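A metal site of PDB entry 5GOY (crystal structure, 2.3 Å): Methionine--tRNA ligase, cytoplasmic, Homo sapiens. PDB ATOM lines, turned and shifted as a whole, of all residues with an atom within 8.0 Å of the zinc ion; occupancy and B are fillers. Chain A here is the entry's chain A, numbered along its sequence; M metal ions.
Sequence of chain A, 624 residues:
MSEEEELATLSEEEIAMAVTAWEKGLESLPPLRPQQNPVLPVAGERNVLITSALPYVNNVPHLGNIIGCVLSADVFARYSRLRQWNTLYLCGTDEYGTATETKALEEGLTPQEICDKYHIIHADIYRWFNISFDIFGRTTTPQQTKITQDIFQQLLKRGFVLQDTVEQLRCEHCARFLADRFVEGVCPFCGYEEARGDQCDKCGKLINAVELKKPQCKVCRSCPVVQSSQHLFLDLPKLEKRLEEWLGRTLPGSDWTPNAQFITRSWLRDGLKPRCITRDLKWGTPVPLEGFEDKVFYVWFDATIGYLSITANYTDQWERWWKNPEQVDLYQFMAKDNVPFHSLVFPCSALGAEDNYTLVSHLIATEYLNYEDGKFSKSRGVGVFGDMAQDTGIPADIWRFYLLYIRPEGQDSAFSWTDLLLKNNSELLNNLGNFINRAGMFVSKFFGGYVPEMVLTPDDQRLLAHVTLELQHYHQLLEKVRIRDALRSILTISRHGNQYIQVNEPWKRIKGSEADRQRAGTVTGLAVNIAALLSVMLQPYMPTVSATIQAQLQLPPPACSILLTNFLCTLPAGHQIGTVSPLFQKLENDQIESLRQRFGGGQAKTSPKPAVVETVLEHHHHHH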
ATOM      1  N   VAL A 186     -19.207   4.816  22.532  1.00  0.00           N
ATOM      2  CA  VAL A 186     -19.553   4.471  23.901  1.00  0.00           C
ATOM      3  C   VAL A 186     -19.807   5.732  24.742  1.00  0.00           C
ATOM      4  O   VAL A 186     -19.088   6.724  24.648  1.00  0.00           O
ATOM      5  CB  VAL A 186     -18.452   3.588  24.564  1.00  0.00           C
ATOM      6  CG1 VAL A 186     -17.068   4.134  24.282  1.00  0.00           C
ATOM      7  CG2 VAL A 186     -18.675   3.430  26.061  1.00  0.00           C
ATOM      8  N   CYS A 187     -20.867   5.660  25.549  1.00  0.00           N
ATOM      9  CA  CYS A 187     -21.351   6.814  26.308  1.00  0.00           C
ATOM     10  C   CYS A 187     -20.403   7.246  27.422  1.00  0.00           C
ATOM     11  O   CYS A 187     -20.005   6.442  28.263  1.00  0.00           O
ATOM     12  CB  CYS A 187     -22.725   6.486  26.893  1.00  0.00           C
ATOM     13  SG  CYS A 187     -23.486   7.871  27.754  1.00  0.00           S
ATOM     14  N   PRO A 188     -20.053   8.547  27.437  1.00  0.00           N
ATOM     15  CA  PRO A 188     -19.170   9.108  28.465  1.00  0.00           C
ATOM     16  C   PRO A 188     -19.890   9.335  29.794  1.00  0.00           C
ATOM     17  O   PRO A 188     -19.264   9.794  30.753  1.00  0.00           O
ATOM     18  CB  PRO A 188     -18.735  10.440  27.853  1.00  0.00           C
ATOM     19  CG  PRO A 188     -19.888  10.831  26.982  1.00  0.00           C
ATOM     20  CD  PRO A 188     -20.423   9.545  26.425  1.00  0.00           C
ATOM     21  N   PHE A 189     -21.180   9.021  29.852  1.00  0.00           N
ATOM     22  CA  PHE A 189     -21.954   9.223  31.073  1.00  0.00           C
ATOM     23  C   PHE A 189     -22.316   7.915  31.777  1.00  0.00           C
ATOM     24  O   PHE A 189     -22.333   7.850  33.003  1.00  0.00           O
ATOM     25  CB  PHE A 189     -23.228  10.017  30.784  1.00  0.00           C
ATOM     26  CG  PHE A 189     -22.970  11.458  30.432  1.00  0.00           C
ATOM     27  CD1 PHE A 189     -22.803  12.405  31.424  1.00  0.00           C
ATOM     28  CD2 PHE A 189     -22.880  11.854  29.111  1.00  0.00           C
ATOM     29  CE1 PHE A 189     -22.571  13.736  31.109  1.00  0.00           C
ATOM     30  CE2 PHE A 189     -22.635  13.180  28.785  1.00  0.00           C
ATOM     31  CZ  PHE A 189     -22.479  14.115  29.789  1.00  0.00           C
ATOM     32  N   CYS A 190     -22.603   6.863  31.005  1.00  0.00           N
ATOM     33  CA  CYS A 190     -22.989   5.594  31.608  1.00  0.00           C
ATOM     34  C   CYS A 190     -22.188   4.392  31.079  1.00  0.00           C
ATOM     35  O   CYS A 190     -22.257   3.303  31.646  1.00  0.00           O
ATOM     36  CB  CYS A 190     -24.488   5.341  31.397  1.00  0.00           C
ATOM     37  SG  CYS A 190     -24.944   4.799  29.745  1.00  0.00           S
ATOM     38  N   GLY A 191     -21.440   4.601  29.999  1.00  0.00           N
ATOM     39  CA  GLY A 191     -20.600   3.548  29.451  1.00  0.00           C
ATOM     40  C   GLY A 191     -21.272   2.660  28.417  1.00  0.00           C
ATOM     41  O   GLY A 191     -20.684   1.666  27.978  1.00  0.00           O
ATOM     42  N   TYR A 192     -22.500   2.998  28.027  1.00  0.00           N
ATOM     43  CA  TYR A 192     -23.220   2.251  27.003  1.00  0.00           C
ATOM     44  C   TYR A 192     -22.421   2.236  25.702  1.00  0.00           C
ATOM     45  O   TYR A 192     -22.205   3.273  25.086  1.00  0.00           O
ATOM     46  CB  TYR A 192     -24.610   2.851  26.770  1.00  0.00           C
ATOM     47  CG  TYR A 192     -25.441   2.087  25.760  1.00  0.00           C
ATOM     48  CD1 TYR A 192     -25.809   0.771  25.980  1.00  0.00           C
ATOM     49  CD2 TYR A 192     -25.897   2.708  24.602  1.00  0.00           C
ATOM     50  CE1 TYR A 192     -26.584   0.071  25.069  1.00  0.00           C
ATOM     51  CE2 TYR A 192     -26.675   2.019  23.681  1.00  0.00           C
ATOM     52  CZ  TYR A 192     -27.011   0.708  23.920  1.00  0.00           C
ATOM     53  OH  TYR A 192     -27.774   0.027  23.004  1.00  0.00           O
ATOM     54  N   GLU A 193     -21.990   1.039  25.289  1.00  0.00           N
ATOM     55  CA  GLU A 193     -21.012   0.895  24.212  1.00  0.00           C
ATOM     56  C   GLU A 193     -21.555   1.180  22.814  1.00  0.00           C
ATOM     57  O   GLU A 193     -20.779   1.259  21.852  1.00  0.00           O
ATOM     58  CB  GLU A 193     -20.422  -0.523  24.249  1.00  0.00           C
ATOM     59  CG  GLU A 193     -19.330  -0.709  25.279  1.00  0.00           C
ATOM     60  CD  GLU A 193     -18.798  -2.130  25.309  1.00  0.00           C
ATOM     61  OE1 GLU A 193     -19.528  -3.044  24.867  1.00  0.00           O
ATOM     62  OE2 GLU A 193     -17.661  -2.328  25.784  1.00  0.00           O
ATOM     63  N   ALA A 195     -23.843   3.898  21.818  1.00  0.00           N
ATOM     64  CA  ALA A 195     -24.587   5.141  21.837  1.00  0.00           C
ATOM     65  C   ALA A 195     -24.510   5.842  20.480  1.00  0.00           C
ATOM     66  O   ALA A 195     -23.575   5.623  19.710  1.00  0.00           O
ATOM     67  CB  ALA A 195     -24.070   6.060  22.941  1.00  0.00           C
ATOM     68  N   GLN A 199     -27.626  11.053  20.993  1.00  0.00           N
ATOM     69  CA  GLN A 199     -28.239  10.623  22.250  1.00  0.00           C
ATOM     70  C   GLN A 199     -27.812   9.208  22.642  1.00  0.00           C
ATOM     71  O   GLN A 199     -27.590   8.353  21.798  1.00  0.00           O
ATOM     72  CB  GLN A 199     -29.757  10.701  22.145  1.00  0.00           C
ATOM     73  CG  GLN A 199     -30.498  10.496  23.453  1.00  0.00           C
ATOM     74  CD  GLN A 199     -32.003  10.521  23.273  1.00  0.00           C
ATOM     75  OE1 GLN A 199     -32.512  10.409  22.158  1.00  0.00           O
ATOM     76  NE2 GLN A 199     -32.729  10.663  24.380  1.00  0.00           N
ATOM     77  N   CYS A 200     -27.711   8.979  23.953  1.00  0.00           N
ATOM     78  CA  CYS A 200     -27.539   7.638  24.481  1.00  0.00           C
ATOM     79  C   CYS A 200     -28.888   7.084  24.904  1.00  0.00           C
ATOM     80  O   CYS A 200     -29.501   7.594  25.837  1.00  0.00           O
ATOM     81  CB  CYS A 200     -26.561   7.637  25.653  1.00  0.00           C
ATOM     82  SG  CYS A 200     -26.446   6.065  26.524  1.00  0.00           S
ATOM     83  N   ASP A 201     -29.362   6.043  24.223  1.00  0.00           N
ATOM     84  CA  ASP A 201     -30.677   5.471  24.509  1.00  0.00           C
ATOM     85  C   ASP A 201     -30.725   4.742  25.848  1.00  0.00           C
ATOM     86  O   ASP A 201     -31.798   4.392  26.340  1.00  0.00           O
ATOM     87  CB  ASP A 201     -31.091   4.510  23.392  1.00  0.00           C
ATOM     88  CG  ASP A 201     -31.430   5.222  22.096  1.00  0.00           C
ATOM     89  OD1 ASP A 201     -31.935   6.374  22.148  1.00  0.00           O
ATOM     90  OD2 ASP A 201     -31.191   4.629  21.021  1.00  0.00           O
ATOM     91  N   LYS A 202     -29.562   4.526  26.446  1.00  0.00           N
ATOM     92  CA  LYS A 202     -29.483   3.746  27.668  1.00  0.00           C
ATOM     93  C   LYS A 202     -29.701   4.613  28.912  1.00  0.00           C
ATOM     94  O   LYS A 202     -30.471   4.244  29.800  1.00  0.00           O
ATOM     95  CB  LYS A 202     -28.133   3.031  27.753  1.00  0.00           C
ATOM     96  CG  LYS A 202     -28.066   1.949  28.805  1.00  0.00           C
ATOM     97  CD  LYS A 202     -29.059   0.837  28.545  1.00  0.00           C
ATOM     98  CE  LYS A 202     -29.035  -0.190  29.660  1.00  0.00           C
ATOM     99  NZ  LYS A 202     -30.034  -1.266  29.464  1.00  0.00           N
ATOM    100  N   CYS A 203     -29.032   5.757  28.970  1.00  0.00           N
ATOM    101  CA  CYS A 203     -29.196   6.664  30.103  1.00  0.00           C
ATOM    102  C   CYS A 203     -29.991   7.912  29.711  1.00  0.00           C
ATOM    103  O   CYS A 203     -30.280   8.770  30.546  1.00  0.00           O
ATOM    104  CB  CYS A 203     -27.838   7.076  30.672  1.00  0.00           C
ATOM    105  SG  CYS A 203     -26.886   8.173  29.623  1.00  0.00           S
ATOM    106  N   GLY A 204     -30.342   8.010  28.426  1.00  0.00           N
ATOM    107  CA  GLY A 204     -31.203   9.063  27.935  1.00  0.00           C
ATOM    108  C   GLY A 204     -30.508  10.371  27.607  1.00  0.00           C
ATOM    109  O   GLY A 204     -31.109  11.253  26.988  1.00  0.00           O
ATOM    110  N   LYS A 205     -29.237  10.489  27.994  1.00  0.00           N
ATOM    111  CA  LYS A 205     -28.502  11.744  27.887  1.00  0.00           C
ATOM    112  C   LYS A 205     -28.379  12.279  26.461  1.00  0.00           C
ATOM    113  O   LYS A 205     -27.884  11.586  25.575  1.00  0.00           O
ATOM    114  CB  LYS A 205     -27.113  11.590  28.486  1.00  0.00           C
ATOM    115  CG  LYS A 205     -26.337  12.889  28.609  1.00  0.00           C
ATOM    116  CD  LYS A 205     -26.747  13.652  29.859  1.00  0.00           C
ATOM    117  CE  LYS A 205     -25.907  14.905  30.031  1.00  0.00           C
ATOM    118  NZ  LYS A 205     -26.191  15.577  31.326  1.00  0.00           N
ATOM    119  N   LEU A 206     -28.834  13.506  26.246  1.00  0.00           N
ATOM    120  CA  LEU A 206     -28.593  14.209  24.993  1.00  0.00           C
ATOM    121  C   LEU A 206     -27.145  14.675  24.928  1.00  0.00           C
ATOM    122  O   LEU A 206     -26.709  15.456  25.773  1.00  0.00           O
ATOM    123  CB  LEU A 206     -29.532  15.409  24.840  1.00  0.00           C
ATOM    124  CG  LEU A 206     -30.979  15.115  24.471  1.00  0.00           C
ATOM    125  CD1 LEU A 206     -31.770  16.406  24.341  1.00  0.00           C
ATOM    126  CD2 LEU A 206     -31.044  14.308  23.174  1.00  0.00           C
ATOM    127  N   ILE A 207     -26.408  14.197  23.940  1.00  0.00           N
ATOM    128  CA  ILE A 207     -24.987  14.506  23.847  1.00  0.00           C
ATOM    129  C   ILE A 207     -24.603  15.085  22.489  1.00  0.00           C
ATOM    130  O   ILE A 207     -25.362  15.025  21.529  1.00  0.00           O
ATOM    131  CB  ILE A 207     -24.136  13.245  24.079  1.00  0.00           C
ATOM    132  CG1 ILE A 207     -24.352  12.242  22.953  1.00  0.00           C
ATOM    133  CG2 ILE A 207     -24.445  12.622  25.429  1.00  0.00           C
ATOM    134  CD1 ILE A 207     -23.202  11.300  22.748  1.00  0.00           C
ATOM    135  N   LEU A 212     -18.423  11.544  22.486  1.00  0.00           N
ATOM    136  CA  LEU A 212     -18.364  10.089  22.448  1.00  0.00           C
ATOM    137  C   LEU A 212     -16.960   9.546  22.599  1.00  0.00           C
ATOM    138  O   LEU A 212     -16.009  10.070  22.013  1.00  0.00           O
ATOM    139  CB  LEU A 212     -18.972   9.563  21.139  1.00  0.00           C
ATOM    140  CG  LEU A 212     -20.489   9.407  21.074  1.00  0.00           C
ATOM    141  CD1 LEU A 212     -20.910   8.906  19.694  1.00  0.00           C
ATOM    142  CD2 LEU A 212     -20.985   8.468  22.162  1.00  0.00           C
HETATM  143 ZN    ZN M   1     -25.332   6.726  28.531  1.00  0.00          ZN
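The backbone carbonyl oxygen (O) of Tyr 192 is in hydrogen-bond range of the backbone NH (N) of Cys 187 (2.8 Å).
The side-chain sulfur (SG) of Cys 187 lies close to the backbone NH (N) of Phe 189.
The backbone NH (N) of Tyr 192 lies close to the side-chain sulfur (SG) of Cys 190 (3.5 Å).
SG of Cys 203 sits close to N of Lys 205, at 3.7 Å.
The backbone NH (N) of Lys 202 sits close to the side-chain sulfur (SG) of Cys 200, 3.5 Å away.
The backbone carbonyl oxygen (O) of Lys 205 is in hydrogen-bond range of the backbone NH (N) of Cys 200, at 3.1 Å.
The zinc ion is bound by the side-chain sulfur (SG) of Cys 187 (2.3 Å).
The zinc ion is bound by SG of Cys 190 (2.3 Å).
The zinc ion is bound by SG of Cys 203 (2.4 Å).
SG of Cys 200 is bound to the zinc ion (2.4 Å).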
